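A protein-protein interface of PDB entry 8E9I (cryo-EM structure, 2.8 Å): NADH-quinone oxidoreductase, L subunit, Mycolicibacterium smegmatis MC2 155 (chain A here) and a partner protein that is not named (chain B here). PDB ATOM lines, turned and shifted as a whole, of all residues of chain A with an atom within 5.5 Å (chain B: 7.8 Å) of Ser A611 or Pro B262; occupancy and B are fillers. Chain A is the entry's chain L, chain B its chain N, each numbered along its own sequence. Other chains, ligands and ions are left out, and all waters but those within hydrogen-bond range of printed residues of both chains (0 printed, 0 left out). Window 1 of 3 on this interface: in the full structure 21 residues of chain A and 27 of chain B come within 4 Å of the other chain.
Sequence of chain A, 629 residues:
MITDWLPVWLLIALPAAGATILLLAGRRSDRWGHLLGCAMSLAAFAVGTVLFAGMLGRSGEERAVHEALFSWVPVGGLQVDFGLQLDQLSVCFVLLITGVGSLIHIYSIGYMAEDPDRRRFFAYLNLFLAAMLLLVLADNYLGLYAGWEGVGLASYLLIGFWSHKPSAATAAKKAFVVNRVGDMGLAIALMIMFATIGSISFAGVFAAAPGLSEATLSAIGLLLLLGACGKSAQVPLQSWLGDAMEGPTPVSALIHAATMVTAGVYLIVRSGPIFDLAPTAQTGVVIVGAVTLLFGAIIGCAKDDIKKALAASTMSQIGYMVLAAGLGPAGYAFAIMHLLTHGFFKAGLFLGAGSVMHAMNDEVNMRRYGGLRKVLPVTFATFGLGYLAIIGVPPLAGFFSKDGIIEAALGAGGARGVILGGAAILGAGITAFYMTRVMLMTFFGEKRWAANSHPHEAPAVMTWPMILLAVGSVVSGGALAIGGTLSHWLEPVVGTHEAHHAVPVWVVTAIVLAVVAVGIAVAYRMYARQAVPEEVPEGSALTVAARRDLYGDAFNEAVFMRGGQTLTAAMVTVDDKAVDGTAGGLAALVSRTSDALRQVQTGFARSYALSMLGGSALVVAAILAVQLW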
ATOM      1  N   VAL A 600     -20.753  -9.711  -2.518  1.00  0.00           N
ATOM      2  CA  VAL A 600     -20.442 -11.135  -2.434  1.00  0.00           C
ATOM      3  C   VAL A 600     -19.861 -11.483  -1.072  1.00  0.00           C
ATOM      4  O   VAL A 600     -19.944 -12.634  -0.629  1.00  0.00           O
ATOM      5  CB  VAL A 600     -19.493 -11.544  -3.575  1.00  0.00           C
ATOM      6  CG1 VAL A 600     -19.131 -13.014  -3.471  1.00  0.00           C
ATOM      7  CG2 VAL A 600     -20.136 -11.246  -4.915  1.00  0.00           C
ATOM      8  N   ARG A 606     -20.030 -19.484   6.109  1.00  0.00           N
ATOM      9  CA  ARG A 606     -20.512 -20.579   5.284  1.00  0.00           C
ATOM     10  C   ARG A 606     -20.664 -20.153   3.833  1.00  0.00           C
ATOM     11  O   ARG A 606     -20.508 -20.976   2.930  1.00  0.00           O
ATOM     12  CB  ARG A 606     -21.827 -21.101   5.847  1.00  0.00           C
ATOM     13  CG  ARG A 606     -21.677 -21.673   7.242  1.00  0.00           C
ATOM     14  CD  ARG A 606     -22.922 -22.377   7.697  1.00  0.00           C
ATOM     15  NE  ARG A 606     -24.100 -21.536   7.525  1.00  0.00           N
ATOM     16  CZ  ARG A 606     -25.209 -21.902   6.899  1.00  0.00           C
ATOM     17  NH1 ARG A 606     -25.362 -23.122   6.408  1.00  0.00           N
ATOM     18  NH2 ARG A 606     -26.196 -21.023   6.766  1.00  0.00           N
ATOM     19  N   SER A 607     -20.938 -18.873   3.576  1.00  0.00           N
ATOM     20  CA  SER A 607     -20.941 -18.403   2.195  1.00  0.00           C
ATOM     21  C   SER A 607     -19.536 -18.395   1.611  1.00  0.00           C
ATOM     22  O   SER A 607     -19.339 -18.786   0.452  1.00  0.00           O
ATOM     23  CB  SER A 607     -21.556 -17.010   2.117  1.00  0.00           C
ATOM     24  OG  SER A 607     -20.664 -16.038   2.627  1.00  0.00           O
ATOM     25  N   TYR A 608     -18.548 -17.959   2.390  1.00  0.00           N
ATOM     26  CA  TYR A 608     -17.168 -18.043   1.931  1.00  0.00           C
ATOM     27  C   TYR A 608     -16.781 -19.488   1.666  1.00  0.00           C
ATOM     28  O   TYR A 608     -16.112 -19.793   0.670  1.00  0.00           O
ATOM     29  CB  TYR A 608     -16.232 -17.438   2.969  1.00  0.00           C
ATOM     30  CG  TYR A 608     -16.527 -16.009   3.349  1.00  0.00           C
ATOM     31  CD1 TYR A 608     -17.377 -15.220   2.591  1.00  0.00           C
ATOM     32  CD2 TYR A 608     -15.948 -15.450   4.474  1.00  0.00           C
ATOM     33  CE1 TYR A 608     -17.635 -13.920   2.944  1.00  0.00           C
ATOM     34  CE2 TYR A 608     -16.199 -14.159   4.834  1.00  0.00           C
ATOM     35  CZ  TYR A 608     -17.043 -13.397   4.070  1.00  0.00           C
ATOM     36  OH  TYR A 608     -17.283 -12.101   4.443  1.00  0.00           O
ATOM     37  N   ALA A 609     -17.191 -20.389   2.556  1.00  0.00           N
ATOM     38  CA  ALA A 609     -16.926 -21.804   2.349  1.00  0.00           C
ATOM     39  C   ALA A 609     -17.631 -22.312   1.102  1.00  0.00           C
ATOM     40  O   ALA A 609     -17.120 -23.195   0.412  1.00  0.00           O
ATOM     41  CB  ALA A 609     -17.362 -22.599   3.576  1.00  0.00           C
ATOM     42  N   LEU A 610     -18.821 -21.789   0.814  1.00  0.00           N
ATOM     43  CA  LEU A 610     -19.523 -22.184  -0.400  1.00  0.00           C
ATOM     44  C   LEU A 610     -18.748 -21.759  -1.634  1.00  0.00           C
ATOM     45  O   LEU A 610     -18.651 -22.514  -2.606  1.00  0.00           O
ATOM     46  CB  LEU A 610     -20.928 -21.586  -0.412  1.00  0.00           C
ATOM     47  CG  LEU A 610     -21.700 -21.662  -1.728  1.00  0.00           C
ATOM     48  CD1 LEU A 610     -21.901 -23.101  -2.162  1.00  0.00           C
ATOM     49  CD2 LEU A 610     -23.035 -20.963  -1.581  1.00  0.00           C
ATOM     50  N   SER A 611     -18.195 -20.549  -1.617  1.00  0.00           N
ATOM     51  CA  SER A 611     -17.347 -20.127  -2.729  1.00  0.00           C
ATOM     52  C   SER A 611     -16.136 -21.040  -2.859  1.00  0.00           C
ATOM     53  O   SER A 611     -15.781 -21.469  -3.963  1.00  0.00           O
ATOM     54  CB  SER A 611     -16.902 -18.680  -2.540  1.00  0.00           C
ATOM     55  OG  SER A 611     -18.011 -17.804  -2.515  1.00  0.00           O
ATOM     56  N   MET A 612     -15.504 -21.368  -1.737  1.00  0.00           N
ATOM     57  CA  MET A 612     -14.336 -22.237  -1.778  1.00  0.00           C
ATOM     58  C   MET A 612     -14.682 -23.616  -2.327  1.00  0.00           C
ATOM     59  O   MET A 612     -13.920 -24.172  -3.124  1.00  0.00           O
ATOM     60  CB  MET A 612     -13.735 -22.346  -0.379  1.00  0.00           C
ATOM     61  CG  MET A 612     -13.005 -21.080   0.039  1.00  0.00           C
ATOM     62  SD  MET A 612     -11.633 -21.352   1.155  1.00  0.00           S
ATOM     63  CE  MET A 612     -12.423 -22.340   2.397  1.00  0.00           C
ATOM     64  N   LEU A 613     -15.820 -24.183  -1.918  1.00  0.00           N
ATOM     65  CA  LEU A 613     -16.247 -25.479  -2.429  1.00  0.00           C
ATOM     66  C   LEU A 613     -16.621 -25.416  -3.902  1.00  0.00           C
ATOM     67  O   LEU A 613     -16.344 -26.360  -4.645  1.00  0.00           O
ATOM     68  CB  LEU A 613     -17.429 -26.008  -1.618  1.00  0.00           C
ATOM     69  CG  LEU A 613     -17.922 -27.405  -2.001  1.00  0.00           C
ATOM     70  CD1 LEU A 613     -16.814 -28.436  -1.897  1.00  0.00           C
ATOM     71  CD2 LEU A 613     -19.095 -27.807  -1.132  1.00  0.00           C
ATOM     72  N   GLY A 614     -17.260 -24.331  -4.340  1.00  0.00           N
ATOM     73  CA  GLY A 614     -17.421 -24.104  -5.761  1.00  0.00           C
ATOM     74  C   GLY A 614     -16.094 -23.966  -6.467  1.00  0.00           C
ATOM     75  O   GLY A 614     -16.022 -24.136  -7.686  1.00  0.00           O
ATOM     76  N   GLY A 615     -15.037 -23.666  -5.716  1.00  0.00           N
ATOM     77  CA  GLY A 615     -13.685 -23.764  -6.234  1.00  0.00           C
ATOM     78  C   GLY A 615     -13.382 -25.083  -6.916  1.00  0.00           C
ATOM     79  O   GLY A 615     -12.354 -25.186  -7.592  1.00  0.00           O
ATOM     80  N   LEU A 618     -11.906 -25.325 -10.154  1.00  0.00           N
ATOM     81  CA  LEU A 618     -10.524 -25.703 -10.416  1.00  0.00           C
ATOM     82  C   LEU A 618     -10.412 -27.176 -10.772  1.00  0.00           C
ATOM     83  O   LEU A 618      -9.694 -27.539 -11.709  1.00  0.00           O
ATOM     84  CB  LEU A 618      -9.653 -25.395  -9.203  1.00  0.00           C
ATOM     85  CG  LEU A 618      -9.188 -23.950  -9.072  1.00  0.00           C
ATOM     86  CD1 LEU A 618     -10.364 -23.007  -8.950  1.00  0.00           C
ATOM     87  CD2 LEU A 618      -8.268 -23.808  -7.877  1.00  0.00           C
ATOM     88  N   LEU B 202     -12.465 -21.633   7.635  1.00  0.00           N
ATOM     89  CA  LEU B 202     -12.047 -21.686   6.243  1.00  0.00           C
ATOM     90  C   LEU B 202     -10.660 -22.291   6.088  1.00  0.00           C
ATOM     91  O   LEU B 202     -10.405 -22.989   5.103  1.00  0.00           O
ATOM     92  CB  LEU B 202     -12.098 -20.284   5.645  1.00  0.00           C
ATOM     93  CG  LEU B 202     -13.472 -19.632   5.775  1.00  0.00           C
ATOM     94  CD1 LEU B 202     -13.407 -18.148   5.517  1.00  0.00           C
ATOM     95  CD2 LEU B 202     -14.422 -20.283   4.800  1.00  0.00           C
ATOM     96  N   PHE B 205     -11.157 -25.991   6.334  1.00  0.00           N
ATOM     97  CA  PHE B 205     -11.698 -26.432   5.052  1.00  0.00           C
ATOM     98  C   PHE B 205     -10.585 -26.573   4.018  1.00  0.00           C
ATOM     99  O   PHE B 205     -10.436 -27.620   3.368  1.00  0.00           O
ATOM    100  CB  PHE B 205     -12.749 -25.423   4.587  1.00  0.00           C
ATOM    101  CG  PHE B 205     -13.857 -26.007   3.766  1.00  0.00           C
ATOM    102  CD1 PHE B 205     -14.620 -27.056   4.247  1.00  0.00           C
ATOM    103  CD2 PHE B 205     -14.164 -25.476   2.524  1.00  0.00           C
ATOM    104  CE1 PHE B 205     -15.651 -27.574   3.493  1.00  0.00           C
ATOM    105  CE2 PHE B 205     -15.196 -25.993   1.767  1.00  0.00           C
ATOM    106  CZ  PHE B 205     -15.937 -27.048   2.256  1.00  0.00           C
ATOM    107  N   VAL B 252      -6.087 -25.849  -4.346  1.00  0.00           N
ATOM    108  CA  VAL B 252      -7.166 -25.215  -3.594  1.00  0.00           C
ATOM    109  C   VAL B 252      -6.642 -24.696  -2.262  1.00  0.00           C
ATOM    110  O   VAL B 252      -6.845 -23.529  -1.902  1.00  0.00           O
ATOM    111  CB  VAL B 252      -8.328 -26.204  -3.402  1.00  0.00           C
ATOM    112  CG1 VAL B 252      -9.254 -25.733  -2.302  1.00  0.00           C
ATOM    113  CG2 VAL B 252      -9.081 -26.383  -4.706  1.00  0.00           C
ATOM    114  N   LEU B 255      -3.974 -21.863  -2.676  1.00  0.00           N
ATOM    115  CA  LEU B 255      -4.617 -20.629  -3.098  1.00  0.00           C
ATOM    116  C   LEU B 255      -5.392 -19.996  -1.960  1.00  0.00           C
ATOM    117  O   LEU B 255      -5.417 -18.768  -1.840  1.00  0.00           O
ATOM    118  CB  LEU B 255      -5.541 -20.894  -4.280  1.00  0.00           C
ATOM    119  CG  LEU B 255      -4.820 -21.235  -5.578  1.00  0.00           C
ATOM    120  CD1 LEU B 255      -5.831 -21.518  -6.661  1.00  0.00           C
ATOM    121  CD2 LEU B 255      -3.894 -20.120  -5.996  1.00  0.00           C
ATOM    122  N   PHE B 256      -6.039 -20.802  -1.122  1.00  0.00           N
ATOM    123  CA  PHE B 256      -6.611 -20.230   0.088  1.00  0.00           C
ATOM    124  C   PHE B 256      -5.533 -19.536   0.903  1.00  0.00           C
ATOM    125  O   PHE B 256      -5.716 -18.408   1.369  1.00  0.00           O
ATOM    126  CB  PHE B 256      -7.289 -21.302   0.930  1.00  0.00           C
ATOM    127  CG  PHE B 256      -7.643 -20.831   2.304  1.00  0.00           C
ATOM    128  CD1 PHE B 256      -8.870 -20.261   2.555  1.00  0.00           C
ATOM    129  CD2 PHE B 256      -6.738 -20.937   3.342  1.00  0.00           C
ATOM    130  CE1 PHE B 256      -9.194 -19.823   3.813  1.00  0.00           C
ATOM    131  CE2 PHE B 256      -7.059 -20.495   4.599  1.00  0.00           C
ATOM    132  CZ  PHE B 256      -8.289 -19.934   4.834  1.00  0.00           C
ATOM    133  N   GLY B 259      -4.713 -16.520  -0.944  1.00  0.00           N
ATOM    134  CA  GLY B 259      -5.902 -15.691  -1.046  1.00  0.00           C
ATOM    135  C   GLY B 259      -6.356 -15.358  -2.452  1.00  0.00           C
ATOM    136  O   GLY B 259      -6.719 -14.207  -2.720  1.00  0.00           O
ATOM    137  N   ALA B 260      -6.364 -16.335  -3.352  1.00  0.00           N
ATOM    138  CA  ALA B 260      -6.919 -16.113  -4.677  1.00  0.00           C
ATOM    139  C   ALA B 260      -8.421 -15.863  -4.581  1.00  0.00           C
ATOM    140  O   ALA B 260      -9.084 -16.293  -3.636  1.00  0.00           O
ATOM    141  CB  ALA B 260      -6.641 -17.310  -5.580  1.00  0.00           C
ATOM    142  N   VAL B 261      -8.962 -15.157  -5.581  1.00  0.00           N
ATOM    143  CA  VAL B 261     -10.361 -14.724  -5.508  1.00  0.00           C
ATOM    144  C   VAL B 261     -11.316 -15.868  -5.219  1.00  0.00           C
ATOM    145  O   VAL B 261     -12.207 -15.700  -4.374  1.00  0.00           O
ATOM    146  CB  VAL B 261     -10.742 -13.939  -6.768  1.00  0.00           C
ATOM    147  CG1 VAL B 261     -12.249 -13.894  -6.913  1.00  0.00           C
ATOM    148  CG2 VAL B 261     -10.264 -12.524  -6.617  1.00  0.00           C
ATOM    149  N   PRO B 262     -11.217 -17.030  -5.857  1.00  0.00           N
ATOM    150  CA  PRO B 262     -12.131 -18.116  -5.491  1.00  0.00           C
ATOM    151  C   PRO B 262     -12.012 -18.487  -4.035  1.00  0.00           C
ATOM    152  O   PRO B 262     -12.932 -19.102  -3.488  1.00  0.00           O
ATOM    153  CB  PRO B 262     -11.703 -19.268  -6.411  1.00  0.00           C
ATOM    154  CG  PRO B 262     -10.944 -18.623  -7.518  1.00  0.00           C
ATOM    155  CD  PRO B 262     -10.278 -17.429  -6.916  1.00  0.00           C
ATOM    156  N   PHE B 263     -10.917 -18.108  -3.383  1.00  0.00           N
ATOM    157  CA  PHE B 263     -10.616 -18.538  -2.033  1.00  0.00           C
ATOM    158  C   PHE B 263     -10.217 -17.375  -1.138  1.00  0.00           C
ATOM    159  O   PHE B 263      -9.757 -17.599  -0.016  1.00  0.00           O
ATOM    160  CB  PHE B 263      -9.492 -19.572  -2.090  1.00  0.00           C
ATOM    161  CG  PHE B 263      -9.874 -20.810  -2.837  1.00  0.00           C
ATOM    162  CD1 PHE B 263     -10.622 -21.802  -2.238  1.00  0.00           C
ATOM    163  CD2 PHE B 263      -9.505 -20.963  -4.161  1.00  0.00           C
ATOM    164  CE1 PHE B 263     -10.986 -22.925  -2.944  1.00  0.00           C
ATOM    165  CE2 PHE B 263      -9.862 -22.087  -4.869  1.00  0.00           C
ATOM    166  CZ  PHE B 263     -10.599 -23.069  -4.264  1.00  0.00           C
ATOM    167  N   HIS B 264     -10.388 -16.140  -1.610  1.00  0.00           N
ATOM    168  CA  HIS B 264      -9.901 -14.960  -0.907  1.00  0.00           C
ATOM    169  C   HIS B 264     -10.866 -14.445   0.144  1.00  0.00           C
ATOM    170  O   HIS B 264     -10.478 -13.600   0.956  1.00  0.00           O
ATOM    171  CB  HIS B 264      -9.664 -13.837  -1.904  1.00  0.00           C
ATOM    172  CG  HIS B 264     -10.917 -13.114  -2.276  1.00  0.00           C
ATOM    173  ND1 HIS B 264     -11.969 -13.742  -2.907  1.00  0.00           N
ATOM    174  CD2 HIS B 264     -11.297 -11.829  -2.096  1.00  0.00           C
ATOM    175  CE1 HIS B 264     -12.940 -12.870  -3.110  1.00  0.00           C
ATOM    176  NE2 HIS B 264     -12.557 -11.702  -2.626  1.00  0.00           N
ATOM    177  N   SER B 265     -12.109 -14.922   0.151  1.00  0.00           N
ATOM    178  CA  SER B 265     -13.153 -14.227   0.893  1.00  0.00           C
ATOM    179  C   SER B 265     -12.776 -14.023   2.353  1.00  0.00           C
ATOM    180  O   SER B 265     -13.217 -13.053   2.975  1.00  0.00           O
ATOM    181  CB  SER B 265     -14.463 -15.000   0.782  1.00  0.00           C
ATOM    182  OG  SER B 265     -14.940 -14.987  -0.549  1.00  0.00           O
ATOM    183  N   TRP B 266     -11.962 -14.914   2.918  1.00  0.00           N
ATOM    184  CA  TRP B 266     -11.586 -14.767   4.318  1.00  0.00           C
ATOM    185  C   TRP B 266     -10.768 -13.502   4.547  1.00  0.00           C
ATOM    186  O   TRP B 266     -11.003 -12.775   5.518  1.00  0.00           O
ATOM    187  CB  TRP B 266     -10.818 -16.002   4.785  1.00  0.00           C
ATOM    188  CG  TRP B 266      -9.512 -16.221   4.110  1.00  0.00           C
ATOM    189  CD1 TRP B 266      -9.313 -16.738   2.870  1.00  0.00           C
ATOM    190  CD2 TRP B 266      -8.214 -15.961   4.650  1.00  0.00           C
ATOM    191  NE1 TRP B 266      -7.974 -16.806   2.596  1.00  0.00           N
ATOM    192  CE2 TRP B 266      -7.276 -16.338   3.676  1.00  0.00           C
ATOM    193  CE3 TRP B 266      -7.755 -15.442   5.860  1.00  0.00           C
ATOM    194  CZ2 TRP B 266      -5.907 -16.202   3.869  1.00  0.00           C
ATOM    195  CZ3 TRP B 266      -6.398 -15.311   6.051  1.00  0.00           C
ATOM    196  CH2 TRP B 266      -5.489 -15.691   5.063  1.00  0.00           C
ATOM    197  N   VAL B 312      -5.673 -23.222 -15.736  1.00  0.00           N
ATOM    198  CA  VAL B 312      -6.416 -22.975 -14.508  1.00  0.00           C
ATOM    199  C   VAL B 312      -5.875 -21.741 -13.806  1.00  0.00           C
ATOM    200  O   VAL B 312      -6.596 -20.761 -13.597  1.00  0.00           O
ATOM    201  CB  VAL B 312      -6.364 -24.211 -13.595  1.00  0.00           C
ATOM    202  CG1 VAL B 312      -7.321 -24.050 -12.435  1.00  0.00           C
ATOM    203  CG2 VAL B 312      -6.696 -25.459 -14.388  1.00  0.00           C
ATOM    204  N   ALA B 315      -6.919 -18.428 -15.312  1.00  0.00           N
ATOM    205  CA  ALA B 315      -8.219 -17.929 -14.894  1.00  0.00           C
ATOM    206  C   ALA B 315      -8.148 -17.375 -13.483  1.00  0.00           C
ATOM    207  O   ALA B 315      -8.501 -16.214 -13.245  1.00  0.00           O
ATOM    208  CB  ALA B 315      -9.262 -19.040 -14.982  1.00  0.00           C
ATOM    209  N   ILE B 316      -7.630 -18.167 -12.546  1.00  0.00           N
ATOM    210  CA  ILE B 316      -7.512 -17.691 -11.174  1.00  0.00           C
ATOM    211  C   ILE B 316      -6.820 -16.340 -11.157  1.00  0.00           C
ATOM    212  O   ILE B 316      -7.379 -15.343 -10.682  1.00  0.00           O
ATOM    213  CB  ILE B 316      -6.764 -18.719 -10.310  1.00  0.00           C
ATOM    214  CG1 ILE B 316      -7.636 -19.949 -10.092  1.00  0.00           C
ATOM    215  CG2 ILE B 316      -6.380 -18.111  -8.984  1.00  0.00           C
ATOM    216  CD1 ILE B 316      -6.855 -21.212  -9.998  1.00  0.00           C
ATOM    217  N   ALA B 317      -5.619 -16.270 -11.735  1.00  0.00           N
ATOM    218  CA  ALA B 317      -4.902 -15.005 -11.736  1.00  0.00           C
ATOM    219  C   ALA B 317      -5.798 -13.899 -12.259  1.00  0.00           C
ATOM    220  O   ALA B 317      -5.987 -12.875 -11.593  1.00  0.00           O
ATOM    221  CB  ALA B 317      -3.632 -15.115 -12.575  1.00  0.00           C
ATOM    222  N   LEU B 319      -9.116 -13.664 -12.399  1.00  0.00           N
ATOM    223  CA  LEU B 319     -10.074 -13.340 -11.355  1.00  0.00           C
ATOM    224  C   LEU B 319      -9.383 -12.626 -10.212  1.00  0.00           C
ATOM    225  O   LEU B 319      -9.817 -11.550  -9.789  1.00  0.00           O
ATOM    226  CB  LEU B 319     -10.754 -14.608 -10.850  1.00  0.00           C
ATOM    227  CG  LEU B 319     -11.839 -15.202 -11.743  1.00  0.00           C
ATOM    228  CD1 LEU B 319     -12.224 -16.577 -11.234  1.00  0.00           C
ATOM    229  CD2 LEU B 319     -13.043 -14.290 -11.804  1.00  0.00           C
ATOM    230  N   THR B 320      -8.266 -13.184  -9.742  1.00  0.00           N
ATOM    231  CA  THR B 320      -7.597 -12.608  -8.586  1.00  0.00           C
ATOM    232  C   THR B 320      -7.319 -11.132  -8.805  1.00  0.00           C
ATOM    233  O   THR B 320      -7.573 -10.308  -7.922  1.00  0.00           O
ATOM    234  CB  THR B 320      -6.308 -13.360  -8.289  1.00  0.00           C
ATOM    235  OG1 THR B 320      -6.572 -14.767  -8.270  1.00  0.00           O
ATOM    236  CG2 THR B 320      -5.764 -12.947  -6.936  1.00  0.00           C
ATOM    237  N   VAL B 323     -11.365  -9.238  -9.535  1.00  0.00           N
ATOM    238  CA  VAL B 323     -12.230  -9.175  -8.364  1.00  0.00           C
ATOM    239  C   VAL B 323     -11.483  -8.585  -7.185  1.00  0.00           C
ATOM    240  O   VAL B 323     -12.046  -7.802  -6.412  1.00  0.00           O
ATOM    241  CB  VAL B 323     -12.776 -10.575  -8.035  1.00  0.00           C
ATOM    242  CG1 VAL B 323     -13.455 -10.579  -6.682  1.00  0.00           C
ATOM    243  CG2 VAL B 323     -13.736 -11.039  -9.112  1.00  0.00           C
ATOM    244  N   VAL B 343      -5.216  -9.208  -1.696  1.00  0.00           N
ATOM    245  CA  VAL B 343      -5.871 -10.154  -2.591  1.00  0.00           C
ATOM    246  C   VAL B 343      -5.377  -9.949  -4.016  1.00  0.00           C
ATOM    247  O   VAL B 343      -5.040 -10.906  -4.718  1.00  0.00           O
ATOM    248  CB  VAL B 343      -7.399 -10.011  -2.494  1.00  0.00           C
ATOM    249  CG1 VAL B 343      -8.074 -10.829  -3.574  1.00  0.00           C
ATOM    250  CG2 VAL B 343      -7.875 -10.438  -1.128  1.00  0.00           C
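O of Ser A607 sits at hydrogen-bond distance from OG of Ser A611.
O of Leu B255 sits at hydrogen-bond distance from N of Ala B260.
The indole nitrogen (NE1) of Trp B266 lies within hydrogen-bond range of the backbone carbonyl oxygen (O) of Phe B256, 3.0 Å away.
The indole nitrogen of Trp B266 sits close to the backbone carbonyl oxygen of Phe B263 (3.3 Å).
The backbone carbonyl oxygen (O) of Ile B316 sits at hydrogen-bond distance from the side-chain hydroxyl (OG1) of Thr B320, 2.6 Å away.
Ser A611 touches just one residue of chain B: Pro B262.
Pro B262 touches just these residues of chain A: Ser A611 and Met A612.
Of the printed residues of chain B, Tyr A608 touches Leu B202 and Ser B265.
Of the printed residues of chain A, Leu B255 touches Leu A618.
Of the printed residues of chain A, Leu B202 touches Tyr A608, Ala A609 and Met A612.
Printed residues of chain A within 4 Å of Ser B265: Tyr A608.
Of the 21 printed residues of chain B, 9 touch a printed residue of chain A.
Among the printed residues, pairs that only touch across the chains: Tyr A608 with Leu B202 (3.8 Å), Tyr A608 with Ser B265 (3.4 Å), Ala A609 with Leu B202 (3.6 Å), Ala A609 with Phe B205 (3.7 Å), Ser A611 with Pro B262 (3.7 Å), Met A612 with Leu B202 (3.4 Å), Met A612 with Phe B205 (3.6 Å), Met A612 with Phe B256 (3.3 Å), Met A612 with Pro B262 (3.8 Å), Met A612 with Phe B263 (3.2 Å), Gly A615 with Phe B263 (3.7 Å), Leu A618 with Leu B255 (3.6 Å), Leu A618 with Phe B263 (3.8 Å), Leu A618 with Val B312 (3.8 Å) and Leu A618 with Ile B316 (3.6 Å).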
